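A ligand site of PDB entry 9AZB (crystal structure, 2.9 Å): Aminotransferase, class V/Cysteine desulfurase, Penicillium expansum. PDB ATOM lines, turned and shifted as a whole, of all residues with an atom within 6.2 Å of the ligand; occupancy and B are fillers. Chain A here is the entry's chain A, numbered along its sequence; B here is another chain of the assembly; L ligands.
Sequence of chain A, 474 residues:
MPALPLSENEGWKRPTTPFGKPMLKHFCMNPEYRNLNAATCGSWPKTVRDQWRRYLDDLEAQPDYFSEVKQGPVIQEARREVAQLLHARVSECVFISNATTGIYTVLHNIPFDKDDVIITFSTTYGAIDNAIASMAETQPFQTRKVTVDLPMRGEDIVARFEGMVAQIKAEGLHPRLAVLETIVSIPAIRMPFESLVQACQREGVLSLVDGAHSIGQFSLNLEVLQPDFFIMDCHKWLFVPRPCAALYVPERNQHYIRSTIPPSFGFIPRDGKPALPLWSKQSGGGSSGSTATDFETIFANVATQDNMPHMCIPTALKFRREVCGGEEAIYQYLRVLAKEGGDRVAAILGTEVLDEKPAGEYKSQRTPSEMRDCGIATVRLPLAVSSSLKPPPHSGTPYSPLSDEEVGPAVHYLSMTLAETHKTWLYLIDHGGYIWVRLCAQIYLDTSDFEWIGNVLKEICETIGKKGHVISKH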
ATOM      1  N   SER A  97     -28.924 -12.895  -3.587  1.00  0.00           N
ATOM      2  CA  SER A  97     -30.131 -12.989  -2.769  1.00  0.00           C
ATOM      3  C   SER A  97     -29.791 -13.210  -1.302  1.00  0.00           C
ATOM      4  O   SER A  97     -30.344 -12.522  -0.427  1.00  0.00           O
ATOM      5  CB  SER A  97     -31.028 -14.109  -3.285  1.00  0.00           C
ATOM      6  OG  SER A  97     -32.378 -13.823  -2.968  1.00  0.00           O
ATOM      7  N   ASN A  98     -28.928 -14.174  -1.006  1.00  0.00           N
ATOM      8  CA  ASN A  98     -28.453 -14.414   0.346  1.00  0.00           C
ATOM      9  C   ASN A  98     -27.010 -14.889   0.265  1.00  0.00           C
ATOM     10  O   ASN A  98     -26.471 -15.104  -0.828  1.00  0.00           O
ATOM     11  CB  ASN A  98     -29.355 -15.417   1.087  1.00  0.00           C
ATOM     12  CG  ASN A  98     -29.644 -16.672   0.258  1.00  0.00           C
ATOM     13  OD1 ASN A  98     -28.745 -17.420  -0.084  1.00  0.00           O
ATOM     14  ND2 ASN A  98     -30.915 -16.886  -0.040  1.00  0.00           N
ATOM     15  N   ALA A  99     -26.365 -15.033   1.419  1.00  0.00           N
ATOM     16  CA  ALA A  99     -24.970 -15.457   1.474  1.00  0.00           C
ATOM     17  C   ALA A  99     -24.783 -16.822   0.821  1.00  0.00           C
ATOM     18  O   ALA A  99     -24.028 -16.940  -0.159  1.00  0.00           O
ATOM     19  CB  ALA A  99     -24.467 -15.493   2.923  1.00  0.00           C
ATOM     20  N   THR A 100     -25.468 -17.845   1.341  1.00  0.00           N
ATOM     21  CA  THR A 100     -25.375 -19.221   0.857  1.00  0.00           C
ATOM     22  C   THR A 100     -25.422 -19.303  -0.669  1.00  0.00           C
ATOM     23  O   THR A 100     -24.685 -20.091  -1.277  1.00  0.00           O
ATOM     24  CB  THR A 100     -26.501 -20.069   1.483  1.00  0.00           C
ATOM     25  OG1 THR A 100     -26.364 -20.064   2.911  1.00  0.00           O
ATOM     26  CG2 THR A 100     -26.459 -21.523   0.985  1.00  0.00           C
ATOM     27  N   THR A 101     -26.244 -18.459  -1.299  1.00  0.00           N
ATOM     28  CA  THR A 101     -26.231 -18.373  -2.753  1.00  0.00           C
ATOM     29  C   THR A 101     -24.868 -17.918  -3.267  1.00  0.00           C
ATOM     30  O   THR A 101     -24.334 -18.468  -4.241  1.00  0.00           O
ATOM     31  CB  THR A 101     -27.310 -17.412  -3.239  1.00  0.00           C
ATOM     32  OG1 THR A 101     -28.604 -17.982  -3.008  1.00  0.00           O
ATOM     33  CG2 THR A 101     -27.116 -17.146  -4.712  1.00  0.00           C
ATOM     34  N   ILE A 103     -21.724 -17.852  -1.780  1.00  0.00           N
ATOM     35  CA  ILE A 103     -20.635 -18.794  -1.555  1.00  0.00           C
ATOM     36  C   ILE A 103     -20.752 -19.951  -2.516  1.00  0.00           C
ATOM     37  O   ILE A 103     -19.786 -20.337  -3.185  1.00  0.00           O
ATOM     38  CB  ILE A 103     -20.645 -19.286  -0.094  1.00  0.00           C
ATOM     39  CG1 ILE A 103     -20.443 -18.125   0.876  1.00  0.00           C
ATOM     40  CG2 ILE A 103     -19.581 -20.378   0.070  1.00  0.00           C
ATOM     41  CD1 ILE A 103     -21.688 -17.740   1.613  1.00  0.00           C
ATOM     42  N   THR A 123     -15.134 -24.509  12.114  1.00  0.00           N
ATOM     43  CA  THR A 123     -16.006 -23.363  12.291  1.00  0.00           C
ATOM     44  C   THR A 123     -16.790 -23.013  11.031  1.00  0.00           C
ATOM     45  O   THR A 123     -17.641 -22.127  11.080  1.00  0.00           O
ATOM     46  CB  THR A 123     -15.196 -22.139  12.737  1.00  0.00           C
ATOM     47  OG1 THR A 123     -13.909 -22.166  12.123  1.00  0.00           O
ATOM     48  CG2 THR A 123     -15.019 -22.148  14.235  1.00  0.00           C
ATOM     49  N   TYR A 125     -19.445 -22.796   8.172  1.00  0.00           N
ATOM     50  CA  TYR A 125     -20.896 -22.915   8.230  1.00  0.00           C
ATOM     51  C   TYR A 125     -21.346 -24.263   7.691  1.00  0.00           C
ATOM     52  O   TYR A 125     -20.840 -24.757   6.682  1.00  0.00           O
ATOM     53  CB  TYR A 125     -21.548 -21.785   7.426  1.00  0.00           C
ATOM     54  CG  TYR A 125     -22.987 -21.479   7.796  1.00  0.00           C
ATOM     55  CD1 TYR A 125     -23.354 -21.228   9.112  1.00  0.00           C
ATOM     56  CD2 TYR A 125     -23.970 -21.428   6.814  1.00  0.00           C
ATOM     57  CE1 TYR A 125     -24.676 -20.947   9.437  1.00  0.00           C
ATOM     58  CE2 TYR A 125     -25.281 -21.128   7.134  1.00  0.00           C
ATOM     59  CZ  TYR A 125     -25.630 -20.899   8.447  1.00  0.00           C
ATOM     60  OH  TYR A 125     -26.947 -20.620   8.750  1.00  0.00           O
ATOM     61  N   ILE A 128     -22.215 -24.644   4.135  1.00  0.00           N
ATOM     62  CA  ILE A 128     -21.072 -24.663   3.226  1.00  0.00           C
ATOM     63  C   ILE A 128     -20.480 -26.058   3.162  1.00  0.00           C
ATOM     64  O   ILE A 128     -20.175 -26.561   2.077  1.00  0.00           O
ATOM     65  CB  ILE A 128     -20.032 -23.622   3.639  1.00  0.00           C
ATOM     66  CG1 ILE A 128     -20.589 -22.214   3.484  1.00  0.00           C
ATOM     67  CG2 ILE A 128     -18.792 -23.753   2.772  1.00  0.00           C
ATOM     68  CD1 ILE A 128     -19.686 -21.139   4.029  1.00  0.00           C
ATOM     69  N   GLU A 181     -14.303 -17.412   7.236  1.00  0.00           N
ATOM     70  CA  GLU A 181     -15.411 -16.565   7.669  1.00  0.00           C
ATOM     71  C   GLU A 181     -14.885 -15.435   8.539  1.00  0.00           C
ATOM     72  O   GLU A 181     -13.952 -15.628   9.325  1.00  0.00           O
ATOM     73  CB  GLU A 181     -16.476 -17.356   8.441  1.00  0.00           C
ATOM     74  CG  GLU A 181     -15.993 -17.997   9.736  1.00  0.00           C
ATOM     75  CD  GLU A 181     -15.248 -19.295   9.504  1.00  0.00           C
ATOM     76  OE1 GLU A 181     -15.379 -19.879   8.398  1.00  0.00           O
ATOM     77  OE2 GLU A 181     -14.538 -19.749  10.431  1.00  0.00           O
ATOM     78  N   ILE A 183     -16.983 -13.843  10.845  1.00  0.00           N
ATOM     79  CA  ILE A 183     -17.583 -14.195  12.125  1.00  0.00           C
ATOM     80  C   ILE A 183     -18.098 -15.622  12.017  1.00  0.00           C
ATOM     81  O   ILE A 183     -18.763 -15.983  11.038  1.00  0.00           O
ATOM     82  CB  ILE A 183     -18.719 -13.223  12.499  1.00  0.00           C
ATOM     83  CG1 ILE A 183     -18.190 -11.793  12.665  1.00  0.00           C
ATOM     84  CG2 ILE A 183     -19.454 -13.692  13.751  1.00  0.00           C
ATOM     85  CD1 ILE A 183     -17.746 -11.476  14.077  1.00  0.00           C
ATOM     86  N   VAL A 184     -17.770 -16.449  13.014  1.00  0.00           N
ATOM     87  CA  VAL A 184     -18.375 -17.768  13.114  1.00  0.00           C
ATOM     88  C   VAL A 184     -19.863 -17.609  13.395  1.00  0.00           C
ATOM     89  O   VAL A 184     -20.262 -16.766  14.212  1.00  0.00           O
ATOM     90  CB  VAL A 184     -17.681 -18.601  14.203  1.00  0.00           C
ATOM     91  CG1 VAL A 184     -18.306 -19.993  14.306  1.00  0.00           C
ATOM     92  CG2 VAL A 184     -16.185 -18.707  13.923  1.00  0.00           C
ATOM     93  N   SER A 185     -20.705 -18.379  12.692  1.00  0.00           N
ATOM     94  CA  SER A 185     -22.150 -18.271  12.872  1.00  0.00           C
ATOM     95  C   SER A 185     -22.527 -18.484  14.336  1.00  0.00           C
ATOM     96  O   SER A 185     -23.193 -17.657  14.952  1.00  0.00           O
ATOM     97  CB  SER A 185     -22.876 -19.277  11.983  1.00  0.00           C
ATOM     98  OG  SER A 185     -22.869 -20.574  12.548  1.00  0.00           O
ATOM     99  N   ILE A 186     -22.105 -19.621  14.891  1.00  0.00           N
ATOM    100  CA  ILE A 186     -22.222 -19.909  16.318  1.00  0.00           C
ATOM    101  C   ILE A 186     -21.355 -21.118  16.611  1.00  0.00           C
ATOM    102  O   ILE A 186     -21.423 -22.122  15.890  1.00  0.00           O
ATOM    103  CB  ILE A 186     -23.689 -20.123  16.740  1.00  0.00           C
ATOM    104  CG1 ILE A 186     -23.795 -20.314  18.262  1.00  0.00           C
ATOM    105  CG2 ILE A 186     -24.327 -21.280  15.986  1.00  0.00           C
ATOM    106  CD1 ILE A 186     -25.089 -19.763  18.852  1.00  0.00           C
ATOM    107  N   ASP A 210     -16.355 -16.114   3.751  1.00  0.00           N
ATOM    108  CA  ASP A 210     -17.759 -16.032   4.149  1.00  0.00           C
ATOM    109  C   ASP A 210     -17.858 -14.928   5.191  1.00  0.00           C
ATOM    110  O   ASP A 210     -17.863 -15.157   6.408  1.00  0.00           O
ATOM    111  CB  ASP A 210     -18.251 -17.375   4.664  1.00  0.00           C
ATOM    112  CG  ASP A 210     -19.561 -17.274   5.468  1.00  0.00           C
ATOM    113  OD1 ASP A 210     -20.345 -16.313   5.258  1.00  0.00           O
ATOM    114  OD2 ASP A 210     -19.786 -18.162   6.339  1.00  0.00           O
ATOM    115  N   ALA A 212     -20.357 -13.198   6.116  1.00  0.00           N
ATOM    116  CA  ALA A 212     -21.791 -12.936   6.256  1.00  0.00           C
ATOM    117  C   ALA A 212     -22.047 -11.882   7.324  1.00  0.00           C
ATOM    118  O   ALA A 212     -22.813 -10.942   7.111  1.00  0.00           O
ATOM    119  CB  ALA A 212     -22.522 -14.236   6.580  1.00  0.00           C
ATOM    120  N   HIS A 213     -21.406 -12.021   8.487  1.00  0.00           N
ATOM    121  CA  HIS A 213     -21.398 -10.961   9.488  1.00  0.00           C
ATOM    122  C   HIS A 213     -20.150 -10.122   9.234  1.00  0.00           C
ATOM    123  O   HIS A 213     -19.042 -10.507   9.613  1.00  0.00           O
ATOM    124  CB  HIS A 213     -21.370 -11.525  10.909  1.00  0.00           C
ATOM    125  CG  HIS A 213     -22.591 -12.323  11.284  1.00  0.00           C
ATOM    126  ND1 HIS A 213     -22.677 -13.687  11.085  1.00  0.00           N
ATOM    127  CD2 HIS A 213     -23.749 -11.956  11.876  1.00  0.00           C
ATOM    128  CE1 HIS A 213     -23.843 -14.118  11.534  1.00  0.00           C
ATOM    129  NE2 HIS A 213     -24.511 -13.087  12.011  1.00  0.00           N
ATOM    130  N   ASP A 233     -23.734 -10.525   4.112  1.00  0.00           N
ATOM    131  CA  ASP A 233     -25.180 -10.396   4.267  1.00  0.00           C
ATOM    132  C   ASP A 233     -25.501  -8.999   4.772  1.00  0.00           C
ATOM    133  O   ASP A 233     -25.409  -8.720   5.972  1.00  0.00           O
ATOM    134  CB  ASP A 233     -25.731 -11.454   5.220  1.00  0.00           C
ATOM    135  CG  ASP A 233     -26.370 -12.618   4.507  1.00  0.00           C
ATOM    136  OD1 ASP A 233     -26.394 -12.620   3.260  1.00  0.00           O
ATOM    137  OD2 ASP A 233     -26.850 -13.542   5.196  1.00  0.00           O
ATOM    138  N   HIS A 235     -28.242  -7.649   5.288  1.00  0.00           N
ATOM    139  CA  HIS A 235     -29.381  -7.636   6.203  1.00  0.00           C
ATOM    140  C   HIS A 235     -28.992  -8.022   7.623  1.00  0.00           C
ATOM    141  O   HIS A 235     -29.852  -8.123   8.495  1.00  0.00           O
ATOM    142  CB  HIS A 235     -30.491  -8.577   5.719  1.00  0.00           C
ATOM    143  CG  HIS A 235     -30.121 -10.024   5.772  1.00  0.00           C
ATOM    144  ND1 HIS A 235     -29.743 -10.739   4.654  1.00  0.00           N
ATOM    145  CD2 HIS A 235     -30.093 -10.903   6.813  1.00  0.00           C
ATOM    146  CE1 HIS A 235     -29.472 -11.988   5.002  1.00  0.00           C
ATOM    147  NE2 HIS A 235     -29.691 -12.111   6.304  1.00  0.00           N
ATOM    148  N   LYS A 236     -27.714  -8.255   7.864  1.00  0.00           N
ATOM    149  CA  LYS A 236     -27.281  -8.648   9.198  1.00  0.00           C
ATOM    150  C   LYS A 236     -26.842  -7.437  10.036  1.00  0.00           C
ATOM    151  O   LYS A 236     -27.072  -7.419  11.253  1.00  0.00           O
ATOM    152  CB  LYS A 236     -26.164  -9.694   9.098  1.00  0.00           C
ATOM    153  CG  LYS A 236     -26.682 -11.078   8.681  1.00  0.00           C
ATOM    154  CD  LYS A 236     -25.741 -12.256   8.923  1.00  0.00           C
ATOM    155  CE  LYS A 236     -26.411 -13.646   8.882  1.00  0.00           C
ATOM    156  NZ  LYS A 236     -25.494 -14.688   8.444  1.00  0.00           N
ATOM    157  N   PRO A 243     -34.203 -11.092   2.612  1.00  0.00           N
ATOM    158  CA  PRO A 243     -32.778 -11.406   2.470  1.00  0.00           C
ATOM    159  C   PRO A 243     -32.054 -10.383   1.600  1.00  0.00           C
ATOM    160  O   PRO A 243     -32.574  -9.926   0.591  1.00  0.00           O
ATOM    161  CB  PRO A 243     -32.806 -12.793   1.817  1.00  0.00           C
ATOM    162  CG  PRO A 243     -34.023 -12.728   0.934  1.00  0.00           C
ATOM    163  CD  PRO A 243     -35.030 -11.870   1.679  1.00  0.00           C
ATOM    164  N   ARG A 438     -25.743 -16.728  21.986  1.00  0.00           N
ATOM    165  CA  ARG A 438     -25.256 -15.656  21.142  1.00  0.00           C
ATOM    166  C   ARG A 438     -26.030 -14.383  21.448  1.00  0.00           C
ATOM    167  O   ARG A 438     -27.260 -14.352  21.283  1.00  0.00           O
ATOM    168  CB  ARG A 438     -25.379 -16.041  19.674  1.00  0.00           C
ATOM    169  CG  ARG A 438     -24.867 -14.994  18.704  1.00  0.00           C
ATOM    170  CD  ARG A 438     -25.804 -14.819  17.514  1.00  0.00           C
ATOM    171  NE  ARG A 438     -25.781 -15.927  16.570  1.00  0.00           N
ATOM    172  CZ  ARG A 438     -26.533 -15.999  15.472  1.00  0.00           C
ATOM    173  NH1 ARG A 438     -27.395 -15.050  15.159  1.00  0.00           N
ATOM    174  NH2 ARG A 438     -26.402 -17.057  14.667  1.00  0.00           N
ATOM    175  N   VAL B 302     -33.547 -24.742   4.451  1.00  0.00           N
ATOM    176  CA  VAL B 302     -32.939 -24.028   3.336  1.00  0.00           C
ATOM    177  C   VAL B 302     -32.438 -22.694   3.873  1.00  0.00           C
ATOM    178  O   VAL B 302     -32.765 -22.298   4.992  1.00  0.00           O
ATOM    179  CB  VAL B 302     -33.947 -23.850   2.166  1.00  0.00           C
ATOM    180  CG1 VAL B 302     -35.121 -23.003   2.613  1.00  0.00           C
ATOM    181  CG2 VAL B 302     -33.283 -23.289   0.899  1.00  0.00           C
ATOM    182  N   ALA B 303     -31.603 -22.018   3.093  1.00  0.00           N
ATOM    183  CA  ALA B 303     -31.088 -20.709   3.498  1.00  0.00           C
ATOM    184  C   ALA B 303     -32.221 -19.705   3.676  1.00  0.00           C
ATOM    185  O   ALA B 303     -33.398 -20.050   3.544  1.00  0.00           O
ATOM    186  CB  ALA B 303     -30.076 -20.191   2.472  1.00  0.00           C
ATOM    187  N   THR B 304     -31.868 -18.450   3.976  1.00  0.00           N
ATOM    188  CA  THR B 304     -32.875 -17.437   4.301  1.00  0.00           C
ATOM    189  C   THR B 304     -33.841 -17.217   3.146  1.00  0.00           C
ATOM    190  O   THR B 304     -33.454 -17.260   1.971  1.00  0.00           O
ATOM    191  CB  THR B 304     -32.184 -16.116   4.675  1.00  0.00           C
ATOM    192  OG1 THR B 304     -31.174 -16.376   5.660  1.00  0.00           O
ATOM    193  CG2 THR B 304     -33.189 -15.099   5.230  1.00  0.00           C
HETATM  194  N1  LIG L   1     -22.492 -18.412   7.128  1.00  0.00           N
HETATM  195  C1  LIG L   1     -22.463 -17.720   8.243  1.00  0.00           C
HETATM  196  C2  LIG L   1     -21.257 -17.804   9.130  1.00  0.00           C
HETATM  197  C3  LIG L   1     -23.555 -16.917   8.633  1.00  0.00           C
HETATM  198  O1  LIG L   1     -23.422 -16.264   9.779  1.00  0.00           O
HETATM  199  C4  LIG L   1     -24.714 -16.826   7.834  1.00  0.00           C
HETATM  200  C5  LIG L   1     -25.806 -15.939   8.281  1.00  0.00           C
HETATM  201  C6  LIG L   1     -24.713 -17.572   6.626  1.00  0.00           C
HETATM  202  C7  LIG L   1     -23.574 -18.327   6.365  1.00  0.00           C
HETATM  203  C8  LIG L   1     -25.809 -17.661   5.591  1.00  0.00           C
HETATM  204  O2  LIG L   1     -26.684 -16.572   5.565  1.00  0.00           O
HETATM  205  P1  LIG L   1     -28.068 -16.844   4.589  1.00  0.00           P
HETATM  206  O3  LIG L   1     -28.708 -15.465   4.363  1.00  0.00           O
HETATM  207  O4  LIG L   1     -28.797 -17.765   5.554  1.00  0.00           O
HETATM  208  O5  LIG L   1     -27.511 -17.480   3.314  1.00  0.00           O
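The side-chain amino group (NZ) of Lys 236 is bonded to a carbon (C5) of the ligand (1.3 Å).
The side-chain hydroxyl (OG1) of Thr 304 of chain B sits at hydrogen-bond distance from an oxygen (O4) of the ligand, 2.8 Å away.
The side-chain carboxylate (OD2) of Asp 233 lies close to an oxygen (O3) of the ligand (2.8 Å).
A ring nitrogen (ND1) of His 213 lies close to an oxygen (O1) of the ligand, 3.0 Å away.
OD2 of Asp 210 is in hydrogen-bond range of N1 of the ligand (2.8 Å).
The backbone NH (N) of Thr 100 lies within hydrogen-bond range of an oxygen (O5) of the ligand (2.9 Å).
OG1 of Thr 100 lies within hydrogen-bond range of O5 of the ligand (2.9 Å).
O5 of the ligand is in hydrogen-bond range of N of Ala 99.
NZ of Lys 236 lies within salt-bridge range of OD2 of Asp 233.
The backbone carbonyl oxygen (O) of Thr 304 of chain B is in hydrogen-bond range of the side-chain amide nitrogen (ND2) of Asn 98 (3.3 Å).
The side-chain carboxylate (OD1) of Asp 233 lies within hydrogen-bond range of the backbone NH (N) of Ala 99, 3.0 Å away.
N of Asp 233 lies within hydrogen-bond range of O of Ala 212, 3.2 Å away.
The side-chain carboxylate (OD2) of Asp 233 sits close to a ring nitrogen (NE2) of His 235.
The side-chain carboxylate of Asp 210 lies close to the backbone NH of Ala 212.
The side-chain amide oxygen (OD1) of Asn 98 lies within hydrogen-bond range of the backbone NH (N) of Thr 101.
The guanidinium group (NH2) of Arg 438 lies within hydrogen-bond range of the backbone carbonyl oxygen (O) of Ser 185, at 3.3 Å.
Asn 98 touches the ligand (CB to O3, 3.3 Å).
Tyr 125 touches the ligand (CD2 to C7, 3.2 Å).
Ile 183 touches the ligand.
CB of Ser 185 touches C2 of the ligand (3.6 Å).
CB of Ala 212 touches C3 of the ligand, at 3.5 Å.
His 235 touches the ligand.
CB of Ala 303 of chain B touches O5 of the ligand (3.8 Å).
Hydrophobic or aromatic side chains within 4 Å of the ligand: Ala 99, Tyr 125, Ala 212, His 213, His 235 and Ala 303 of chain B.
14 residues have an atom within 4 Å of the ligand: Asn 98, Ala 99, Thr 100, Tyr 125, Ile 183, Ser 185, Asp 210, Ala 212, His 213, Asp 233, His 235, Lys 236, Ala 303 of chain B and Thr 304 of chain B.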
